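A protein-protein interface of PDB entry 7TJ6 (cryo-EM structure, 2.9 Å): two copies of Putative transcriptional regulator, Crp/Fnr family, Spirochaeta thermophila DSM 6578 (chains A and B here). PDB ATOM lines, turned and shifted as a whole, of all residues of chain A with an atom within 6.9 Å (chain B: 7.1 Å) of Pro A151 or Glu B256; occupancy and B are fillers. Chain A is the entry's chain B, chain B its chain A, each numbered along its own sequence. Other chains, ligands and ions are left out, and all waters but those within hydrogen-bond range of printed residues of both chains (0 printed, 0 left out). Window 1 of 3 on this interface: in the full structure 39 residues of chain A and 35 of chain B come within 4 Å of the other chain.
No position is printed for both chains.
Among the printed residues, pairs that only touch across the chains: Pro A151 with Glu B256 (3.1 Å), Arg A155 with Arg B252 (3.7 Å) and Tyr A289 with Ala B260 (3.4 Å).
The backbone carbonyl oxygen (O) of Ala B260 sits at hydrogen-bond distance from the side-chain hydroxyl (OG) of Ser B263, at 2.8 Å.
Of chain B, only Glu B256 comes within 4 Å of Pro A151. Of the printed residues of chain A, Glu B256 touches Pro A151 (3.1 Å). Of the printed residues of chain B, Arg A155 touches Arg B252 (3.7 Å). Printed residues of chain B within 4 Å of Tyr A289: Ala B260 (3.4 Å). Of the printed residues of chain A, Ala B260 touches Tyr A289 (3.4 Å). Printed residues of chain A within 4 Å of Arg B252: Arg A155. Leu B262 touches none of the printed residues of chain A. The nearest residue of chain A that does not touch Glu B256 is Arg A155 (4.4 Å). The nearest printed residue of chain B that does not touch Arg A155 is Glu B256 (4.4 Å).
Printed residues of chain A that touch a printed residue of chain B: Pro A151, Arg A155 and Tyr A289. Along chain A the printed residues that touch a printed residue of chain B span positions 151 to 289. Of the 15 printed residues of chain B, 3 touch a printed residue of chain A. Printed residues of chain B that touch a printed residue of chain A: Arg B252, Glu B256 and Ala B260. Hydrophobic or aromatic side chains of chain B that line the printed part of chain A: Ala B260. Among the printed residues, 3 pairs touch across the chains.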
ATOM      1  N   THR A 142     -30.034  14.276   4.027  1.00  0.00           N
ATOM      2  CA  THR A 142     -29.366  13.811   2.815  1.00  0.00           C
ATOM      3  C   THR A 142     -30.033  14.380   1.569  1.00  0.00           C
ATOM      4  O   THR A 142     -29.353  14.740   0.600  1.00  0.00           O
ATOM      5  CB  THR A 142     -29.371  12.284   2.759  1.00  0.00           C
ATOM      6  OG1 THR A 142     -30.688  11.800   3.047  1.00  0.00           O
ATOM      7  CG2 THR A 142     -28.399  11.703   3.774  1.00  0.00           C
ATOM      8  N   LEU A 145     -29.571  18.853   1.920  1.00  0.00           N
ATOM      9  CA  LEU A 145     -28.264  19.502   1.919  1.00  0.00           C
ATOM     10  C   LEU A 145     -27.371  19.110   0.746  1.00  0.00           C
ATOM     11  O   LEU A 145     -26.297  19.701   0.588  1.00  0.00           O
ATOM     12  CB  LEU A 145     -27.559  19.210   3.247  1.00  0.00           C
ATOM     13  CG  LEU A 145     -28.150  19.756   4.546  1.00  0.00           C
ATOM     14  CD1 LEU A 145     -27.387  19.233   5.752  1.00  0.00           C
ATOM     15  CD2 LEU A 145     -28.139  21.278   4.519  1.00  0.00           C
ATOM     16  N   SER A 146     -27.774  18.142  -0.079  1.00  0.00           N
ATOM     17  CA  SER A 146     -26.966  17.732  -1.225  1.00  0.00           C
ATOM     18  C   SER A 146     -26.970  18.737  -2.376  1.00  0.00           C
ATOM     19  O   SER A 146     -26.158  18.591  -3.297  1.00  0.00           O
ATOM     20  CB  SER A 146     -27.449  16.374  -1.742  1.00  0.00           C
ATOM     21  OG  SER A 146     -28.807  16.430  -2.143  1.00  0.00           O
ATOM     22  N   TYR A 147     -27.846  19.747  -2.350  1.00  0.00           N
ATOM     23  CA  TYR A 147     -27.914  20.719  -3.439  1.00  0.00           C
ATOM     24  C   TYR A 147     -26.716  21.659  -3.517  1.00  0.00           C
ATOM     25  O   TYR A 147     -26.535  22.311  -4.551  1.00  0.00           O
ATOM     26  CB  TYR A 147     -29.199  21.541  -3.326  1.00  0.00           C
ATOM     27  CG  TYR A 147     -30.453  20.722  -3.520  1.00  0.00           C
ATOM     28  CD1 TYR A 147     -30.579  19.863  -4.602  1.00  0.00           C
ATOM     29  CD2 TYR A 147     -31.511  20.815  -2.627  1.00  0.00           C
ATOM     30  CE1 TYR A 147     -31.722  19.112  -4.788  1.00  0.00           C
ATOM     31  CE2 TYR A 147     -32.660  20.066  -2.806  1.00  0.00           C
ATOM     32  CZ  TYR A 147     -32.760  19.218  -3.888  1.00  0.00           C
ATOM     33  OH  TYR A 147     -33.900  18.470  -4.073  1.00  0.00           O
ATOM     34  N   ILE A 149     -23.469  21.015  -1.410  1.00  0.00           N
ATOM     35  CA  ILE A 149     -22.171  20.419  -0.962  1.00  0.00           C
ATOM     36  C   ILE A 149     -21.985  19.024  -1.552  1.00  0.00           C
ATOM     37  O   ILE A 149     -22.981  18.403  -1.923  1.00  0.00           O
ATOM     38  CB  ILE A 149     -22.096  20.374   0.574  1.00  0.00           C
ATOM     39  CG1 ILE A 149     -22.052  21.777   1.187  1.00  0.00           C
ATOM     40  CG2 ILE A 149     -20.926  19.518   1.035  1.00  0.00           C
ATOM     41  CD1 ILE A 149     -22.241  21.799   2.686  1.00  0.00           C
ATOM     42  N   ASN A 150     -20.738  18.567  -1.618  1.00  0.00           N
ATOM     43  CA  ASN A 150     -20.465  17.241  -2.199  1.00  0.00           C
ATOM     44  C   ASN A 150     -21.233  16.241  -1.375  1.00  0.00           C
ATOM     45  O   ASN A 150     -21.147  16.307  -0.145  1.00  0.00           O
ATOM     46  CB  ASN A 150     -18.991  16.876  -2.110  1.00  0.00           C
ATOM     47  CG  ASN A 150     -18.097  17.817  -2.890  1.00  0.00           C
ATOM     48  OD1 ASN A 150     -18.578  18.718  -3.575  1.00  0.00           O
ATOM     49  ND2 ASN A 150     -16.793  17.614  -2.795  1.00  0.00           N
ATOM     50  N   PRO A 151     -21.969  15.314  -1.985  1.00  0.00           N
ATOM     51  CA  PRO A 151     -22.802  14.422  -1.215  1.00  0.00           C
ATOM     52  C   PRO A 151     -21.986  13.363  -0.484  1.00  0.00           C
ATOM     53  O   PRO A 151     -22.382  12.990   0.595  1.00  0.00           O
ATOM     54  CB  PRO A 151     -23.710  13.816  -2.285  1.00  0.00           C
ATOM     55  CG  PRO A 151     -23.661  14.850  -3.383  1.00  0.00           C
ATOM     56  CD  PRO A 151     -22.194  15.209  -3.420  1.00  0.00           C
ATOM     57  N   ALA A 152     -20.926  12.877  -1.085  1.00  0.00           N
ATOM     58  CA  ALA A 152     -20.027  11.913  -0.455  1.00  0.00           C
ATOM     59  C   ALA A 152     -19.545  12.429   0.897  1.00  0.00           C
ATOM     60  O   ALA A 152     -19.527  11.688   1.888  1.00  0.00           O
ATOM     61  CB  ALA A 152     -18.844  11.616  -1.375  1.00  0.00           C
ATOM     62  N   LEU A 153     -19.186  13.710   0.966  1.00  0.00           N
ATOM     63  CA  LEU A 153     -18.797  14.303   2.241  1.00  0.00           C
ATOM     64  C   LEU A 153     -19.971  14.296   3.214  1.00  0.00           C
ATOM     65  O   LEU A 153     -19.799  14.026   4.412  1.00  0.00           O
ATOM     66  CB  LEU A 153     -18.276  15.720   2.031  1.00  0.00           C
ATOM     67  CG  LEU A 153     -17.817  16.501   3.260  1.00  0.00           C
ATOM     68  CD1 LEU A 153     -16.541  15.897   3.817  1.00  0.00           C
ATOM     69  CD2 LEU A 153     -17.612  17.963   2.913  1.00  0.00           C
ATOM     70  N   LEU A 154     -21.174  14.605   2.714  1.00  0.00           N
ATOM     71  CA  LEU A 154     -22.346  14.600   3.591  1.00  0.00           C
ATOM     72  C   LEU A 154     -22.638  13.204   4.148  1.00  0.00           C
ATOM     73  O   LEU A 154     -22.979  13.055   5.330  1.00  0.00           O
ATOM     74  CB  LEU A 154     -23.550  15.124   2.807  1.00  0.00           C
ATOM     75  CG  LEU A 154     -24.911  15.405   3.446  1.00  0.00           C
ATOM     76  CD1 LEU A 154     -25.629  16.383   2.551  1.00  0.00           C
ATOM     77  CD2 LEU A 154     -25.750  14.153   3.614  1.00  0.00           C
ATOM     78  N   ARG A 155     -22.491  12.170   3.320  1.00  0.00           N
ATOM     79  CA  ARG A 155     -22.662  10.796   3.782  1.00  0.00           C
ATOM     80  C   ARG A 155     -21.596  10.427   4.807  1.00  0.00           C
ATOM     81  O   ARG A 155     -21.873   9.695   5.766  1.00  0.00           O
ATOM     82  CB  ARG A 155     -22.649   9.838   2.591  1.00  0.00           C
ATOM     83  CG  ARG A 155     -23.861   9.968   1.677  1.00  0.00           C
ATOM     84  CD  ARG A 155     -23.974   8.790   0.718  1.00  0.00           C
ATOM     85  NE  ARG A 155     -22.877   8.766  -0.241  1.00  0.00           N
ATOM     86  CZ  ARG A 155     -22.906   9.364  -1.425  1.00  0.00           C
ATOM     87  NH1 ARG A 155     -23.967  10.041  -1.830  1.00  0.00           N
ATOM     88  NH2 ARG A 155     -21.842   9.286  -2.218  1.00  0.00           N
ATOM     89  N   LEU A 156     -20.364  10.910   4.611  1.00  0.00           N
ATOM     90  CA  LEU A 156     -19.309  10.659   5.593  1.00  0.00           C
ATOM     91  C   LEU A 156     -19.663  11.263   6.943  1.00  0.00           C
ATOM     92  O   LEU A 156     -19.514  10.611   7.990  1.00  0.00           O
ATOM     93  CB  LEU A 156     -17.984  11.227   5.075  1.00  0.00           C
ATOM     94  CG  LEU A 156     -16.645  10.881   5.735  1.00  0.00           C
ATOM     95  CD1 LEU A 156     -15.534  11.019   4.713  1.00  0.00           C
ATOM     96  CD2 LEU A 156     -16.335  11.770   6.933  1.00  0.00           C
ATOM     97  N   LEU A 157     -20.168  12.497   6.935  1.00  0.00           N
ATOM     98  CA  LEU A 157     -20.571  13.134   8.185  1.00  0.00           C
ATOM     99  C   LEU A 157     -21.720  12.378   8.842  1.00  0.00           C
ATOM    100  O   LEU A 157     -21.745  12.210  10.069  1.00  0.00           O
ATOM    101  CB  LEU A 157     -20.973  14.584   7.925  1.00  0.00           C
ATOM    102  CG  LEU A 157     -19.870  15.523   7.439  1.00  0.00           C
ATOM    103  CD1 LEU A 157     -20.452  16.880   7.087  1.00  0.00           C
ATOM    104  CD2 LEU A 157     -18.784  15.662   8.490  1.00  0.00           C
ATOM    105  N   LEU A 240     -16.092   5.796   0.804  1.00  0.00           N
ATOM    106  CA  LEU A 240     -16.529   7.164   0.558  1.00  0.00           C
ATOM    107  C   LEU A 240     -15.354   8.130   0.465  1.00  0.00           C
ATOM    108  O   LEU A 240     -15.395   9.087  -0.318  1.00  0.00           O
ATOM    109  CB  LEU A 240     -17.503   7.563   1.651  1.00  0.00           C
ATOM    110  CG  LEU A 240     -18.571   8.579   1.319  1.00  0.00           C
ATOM    111  CD1 LEU A 240     -19.472   8.043   0.235  1.00  0.00           C
ATOM    112  CD2 LEU A 240     -19.339   8.662   2.578  1.00  0.00           C
ATOM    113  N   TYR A 289     -12.405  15.629 -17.395  1.00  0.00           N
ATOM    114  CA  TYR A 289     -13.821  15.270 -17.626  1.00  0.00           C
ATOM    115  C   TYR A 289     -13.978  15.221 -19.138  1.00  0.00           C
ATOM    116  O   TYR A 289     -14.065  16.295 -19.749  1.00  0.00           O
ATOM    117  CB  TYR A 289     -14.774  16.297 -17.014  1.00  0.00           C
ATOM    118  CG  TYR A 289     -15.113  16.141 -15.556  1.00  0.00           C
ATOM    119  CD1 TYR A 289     -15.958  15.136 -15.120  1.00  0.00           C
ATOM    120  CD2 TYR A 289     -14.640  17.043 -14.621  1.00  0.00           C
ATOM    121  CE1 TYR A 289     -16.290  15.004 -13.783  1.00  0.00           C
ATOM    122  CE2 TYR A 289     -14.961  16.926 -13.280  1.00  0.00           C
ATOM    123  CZ  TYR A 289     -15.792  15.904 -12.860  1.00  0.00           C
ATOM    124  OH  TYR A 289     -16.110  15.784 -11.538  1.00  0.00           O
ATOM    125  N   LEU B 250     -27.185   2.884  -8.675  1.00  0.00           N
ATOM    126  CA  LEU B 250     -26.896   3.250 -10.059  1.00  0.00           C
ATOM    127  C   LEU B 250     -27.497   4.601 -10.412  1.00  0.00           C
ATOM    128  O   LEU B 250     -26.834   5.434 -11.051  1.00  0.00           O
ATOM    129  CB  LEU B 250     -27.429   2.182 -11.013  1.00  0.00           C
ATOM    130  CG  LEU B 250     -26.837   0.777 -10.986  1.00  0.00           C
ATOM    131  CD1 LEU B 250     -27.627  -0.137 -11.913  1.00  0.00           C
ATOM    132  CD2 LEU B 250     -25.371   0.814 -11.373  1.00  0.00           C
ATOM    133  N   HIS B 251     -28.733   4.856  -9.971  1.00  0.00           N
ATOM    134  CA  HIS B 251     -29.311   6.174 -10.212  1.00  0.00           C
ATOM    135  C   HIS B 251     -28.466   7.244  -9.544  1.00  0.00           C
ATOM    136  O   HIS B 251     -28.178   8.295 -10.143  1.00  0.00           O
ATOM    137  CB  HIS B 251     -30.750   6.252  -9.715  1.00  0.00           C
ATOM    138  CG  HIS B 251     -31.479   7.462 -10.211  1.00  0.00           C
ATOM    139  ND1 HIS B 251     -32.054   7.524 -11.461  1.00  0.00           N
ATOM    140  CD2 HIS B 251     -31.685   8.672  -9.642  1.00  0.00           C
ATOM    141  CE1 HIS B 251     -32.606   8.711 -11.632  1.00  0.00           C
ATOM    142  NE2 HIS B 251     -32.392   9.429 -10.544  1.00  0.00           N
ATOM    143  N   ARG B 252     -28.055   6.990  -8.300  1.00  0.00           N
ATOM    144  CA  ARG B 252     -27.318   8.000  -7.560  1.00  0.00           C
ATOM    145  C   ARG B 252     -25.965   8.263  -8.204  1.00  0.00           C
ATOM    146  O   ARG B 252     -25.565   9.417  -8.342  1.00  0.00           O
ATOM    147  CB  ARG B 252     -27.152   7.564  -6.108  1.00  0.00           C
ATOM    148  CG  ARG B 252     -27.043   8.705  -5.121  1.00  0.00           C
ATOM    149  CD  ARG B 252     -26.976   8.175  -3.700  1.00  0.00           C
ATOM    150  NE  ARG B 252     -25.840   7.279  -3.517  1.00  0.00           N
ATOM    151  CZ  ARG B 252     -25.616   6.570  -2.420  1.00  0.00           C
ATOM    152  NH1 ARG B 252     -26.435   6.623  -1.383  1.00  0.00           N
ATOM    153  NH2 ARG B 252     -24.549   5.776  -2.368  1.00  0.00           N
ATOM    154  N   GLU B 253     -25.271   7.218  -8.666  1.00  0.00           N
ATOM    155  CA  GLU B 253     -23.951   7.435  -9.250  1.00  0.00           C
ATOM    156  C   GLU B 253     -24.043   8.147 -10.596  1.00  0.00           C
ATOM    157  O   GLU B 253     -23.203   9.011 -10.896  1.00  0.00           O
ATOM    158  CB  GLU B 253     -23.201   6.105  -9.376  1.00  0.00           C
ATOM    159  CG  GLU B 253     -23.725   5.152 -10.443  1.00  0.00           C
ATOM    160  CD  GLU B 253     -22.944   3.851 -10.512  1.00  0.00           C
ATOM    161  OE1 GLU B 253     -22.280   3.500  -9.514  1.00  0.00           O
ATOM    162  OE2 GLU B 253     -22.996   3.178 -11.563  1.00  0.00           O
ATOM    163  N   ARG B 254     -25.115   7.900 -11.359  1.00  0.00           N
ATOM    164  CA  ARG B 254     -25.274   8.588 -12.637  1.00  0.00           C
ATOM    165  C   ARG B 254     -25.529  10.070 -12.405  1.00  0.00           C
ATOM    166  O   ARG B 254     -24.856  10.938 -12.989  1.00  0.00           O
ATOM    167  CB  ARG B 254     -26.415   7.958 -13.436  1.00  0.00           C
ATOM    168  CG  ARG B 254     -26.040   6.668 -14.148  1.00  0.00           C
ATOM    169  CD  ARG B 254     -27.232   6.033 -14.854  1.00  0.00           C
ATOM    170  NE  ARG B 254     -27.885   6.939 -15.791  1.00  0.00           N
ATOM    171  CZ  ARG B 254     -29.131   7.374 -15.663  1.00  0.00           C
ATOM    172  NH1 ARG B 254     -29.889   7.007 -14.642  1.00  0.00           N
ATOM    173  NH2 ARG B 254     -29.629   8.198 -16.580  1.00  0.00           N
ATOM    174  N   VAL B 255     -26.484  10.375 -11.526  1.00  0.00           N
ATOM    175  CA  VAL B 255     -26.834  11.764 -11.272  1.00  0.00           C
ATOM    176  C   VAL B 255     -25.669  12.492 -10.610  1.00  0.00           C
ATOM    177  O   VAL B 255     -25.442  13.678 -10.877  1.00  0.00           O
ATOM    178  CB  VAL B 255     -28.119  11.827 -10.427  1.00  0.00           C
ATOM    179  CG1 VAL B 255     -28.465  13.257 -10.070  1.00  0.00           C
ATOM    180  CG2 VAL B 255     -29.266  11.175 -11.181  1.00  0.00           C
ATOM    181  N   GLU B 256     -24.900  11.802  -9.761  1.00  0.00           N
ATOM    182  CA  GLU B 256     -23.751  12.428  -9.114  1.00  0.00           C
ATOM    183  C   GLU B 256     -22.674  12.798 -10.124  1.00  0.00           C
ATOM    184  O   GLU B 256     -22.101  13.891 -10.051  1.00  0.00           O
ATOM    185  CB  GLU B 256     -23.153  11.497  -8.060  1.00  0.00           C
ATOM    186  CG  GLU B 256     -23.955  11.379  -6.786  1.00  0.00           C
ATOM    187  CD  GLU B 256     -24.035  12.644  -5.991  1.00  0.00           C
ATOM    188  OE1 GLU B 256     -23.182  13.538  -6.168  1.00  0.00           O
ATOM    189  OE2 GLU B 256     -24.992  12.739  -5.199  1.00  0.00           O
ATOM    190  N   ARG B 257     -22.389  11.904 -11.078  1.00  0.00           N
ATOM    191  CA  ARG B 257     -21.403  12.231 -12.106  1.00  0.00           C
ATOM    192  C   ARG B 257     -21.856  13.420 -12.946  1.00  0.00           C
ATOM    193  O   ARG B 257     -21.065  14.339 -13.226  1.00  0.00           O
ATOM    194  CB  ARG B 257     -21.156  11.009 -12.987  1.00  0.00           C
ATOM    195  CG  ARG B 257     -20.004  11.157 -13.957  1.00  0.00           C
ATOM    196  CD  ARG B 257     -19.696   9.838 -14.652  1.00  0.00           C
ATOM    197  NE  ARG B 257     -20.849   9.301 -15.366  1.00  0.00           N
ATOM    198  CZ  ARG B 257     -21.531   8.226 -14.996  1.00  0.00           C
ATOM    199  NH1 ARG B 257     -21.171   7.505 -13.948  1.00  0.00           N
ATOM    200  NH2 ARG B 257     -22.590   7.853 -15.710  1.00  0.00           N
ATOM    201  N   VAL B 258     -23.136  13.436 -13.328  1.00  0.00           N
ATOM    202  CA  VAL B 258     -23.647  14.544 -14.132  1.00  0.00           C
ATOM    203  C   VAL B 258     -23.571  15.861 -13.367  1.00  0.00           C
ATOM    204  O   VAL B 258     -23.133  16.887 -13.907  1.00  0.00           O
ATOM    205  CB  VAL B 258     -25.084  14.251 -14.586  1.00  0.00           C
ATOM    206  CG1 VAL B 258     -25.700  15.502 -15.151  1.00  0.00           C
ATOM    207  CG2 VAL B 258     -25.088  13.144 -15.619  1.00  0.00           C
ATOM    208  N   THR B 259     -23.969  15.849 -12.092  1.00  0.00           N
ATOM    209  CA  THR B 259     -23.946  17.070 -11.295  1.00  0.00           C
ATOM    210  C   THR B 259     -22.525  17.554 -11.042  1.00  0.00           C
ATOM    211  O   THR B 259     -22.280  18.766 -11.030  1.00  0.00           O
ATOM    212  CB  THR B 259     -24.689  16.830  -9.977  1.00  0.00           C
ATOM    213  OG1 THR B 259     -26.082  16.633 -10.247  1.00  0.00           O
ATOM    214  CG2 THR B 259     -24.541  18.015  -9.032  1.00  0.00           C
ATOM    215  N   ALA B 260     -21.570  16.635 -10.878  1.00  0.00           N
ATOM    216  CA  ALA B 260     -20.176  17.041 -10.731  1.00  0.00           C
ATOM    217  C   ALA B 260     -19.673  17.749 -11.983  1.00  0.00           C
ATOM    218  O   ALA B 260     -19.036  18.810 -11.898  1.00  0.00           O
ATOM    219  CB  ALA B 260     -19.307  15.823 -10.415  1.00  0.00           C
ATOM    220  N   PHE B 261     -19.963  17.180 -13.159  1.00  0.00           N
ATOM    221  CA  PHE B 261     -19.601  17.849 -14.409  1.00  0.00           C
ATOM    222  C   PHE B 261     -20.223  19.237 -14.509  1.00  0.00           C
ATOM    223  O   PHE B 261     -19.547  20.213 -14.865  1.00  0.00           O
ATOM    224  CB  PHE B 261     -20.036  17.015 -15.605  1.00  0.00           C
ATOM    225  CG  PHE B 261     -19.768  17.678 -16.920  1.00  0.00           C
ATOM    226  CD1 PHE B 261     -18.471  17.930 -17.326  1.00  0.00           C
ATOM    227  CD2 PHE B 261     -20.812  18.082 -17.736  1.00  0.00           C
ATOM    228  CE1 PHE B 261     -18.216  18.540 -18.534  1.00  0.00           C
ATOM    229  CE2 PHE B 261     -20.563  18.701 -18.943  1.00  0.00           C
ATOM    230  CZ  PHE B 261     -19.263  18.929 -19.342  1.00  0.00           C
ATOM    231  N   LEU B 262     -21.517  19.339 -14.199  1.00  0.00           N
ATOM    232  CA  LEU B 262     -22.212  20.615 -14.338  1.00  0.00           C
ATOM    233  C   LEU B 262     -21.639  21.659 -13.391  1.00  0.00           C
ATOM    234  O   LEU B 262     -21.458  22.821 -13.771  1.00  0.00           O
ATOM    235  CB  LEU B 262     -23.707  20.429 -14.099  1.00  0.00           C
ATOM    236  CG  LEU B 262     -24.429  19.574 -15.139  1.00  0.00           C
ATOM    237  CD1 LEU B 262     -25.890  19.439 -14.774  1.00  0.00           C
ATOM    238  CD2 LEU B 262     -24.268  20.160 -16.532  1.00  0.00           C
ATOM    239  N   SER B 263     -21.344  21.263 -12.153  1.00  0.00           N
ATOM    240  CA  SER B 263     -20.776  22.203 -11.195  1.00  0.00           C
ATOM    241  C   SER B 263     -19.381  22.644 -11.622  1.00  0.00           C
ATOM    242  O   SER B 263     -19.007  23.805 -11.423  1.00  0.00           O
ATOM    243  CB  SER B 263     -20.742  21.574  -9.802  1.00  0.00           C
ATOM    244  OG  SER B 263     -19.880  20.450  -9.774  1.00  0.00           O
ATOM    245  N   PHE B 279     -33.799  14.696 -13.267  1.00  0.00           N
ATOM    246  CA  PHE B 279     -33.290  13.439 -12.730  1.00  0.00           C
ATOM    247  C   PHE B 279     -34.161  12.959 -11.575  1.00  0.00           C
ATOM    248  O   PHE B 279     -34.381  11.753 -11.408  1.00  0.00           O
ATOM    249  CB  PHE B 279     -31.833  13.586 -12.303  1.00  0.00           C
ATOM    250  CG  PHE B 279     -30.865  13.422 -13.436  1.00  0.00           C
ATOM    251  CD1 PHE B 279     -31.002  12.378 -14.333  1.00  0.00           C
ATOM    252  CD2 PHE B 279     -29.831  14.320 -13.618  1.00  0.00           C
ATOM    253  CE1 PHE B 279     -30.125  12.235 -15.389  1.00  0.00           C
ATOM    254  CE2 PHE B 279     -28.948  14.178 -14.671  1.00  0.00           C
ATOM    255  CZ  PHE B 279     -29.095  13.136 -15.556  1.00  0.00           C
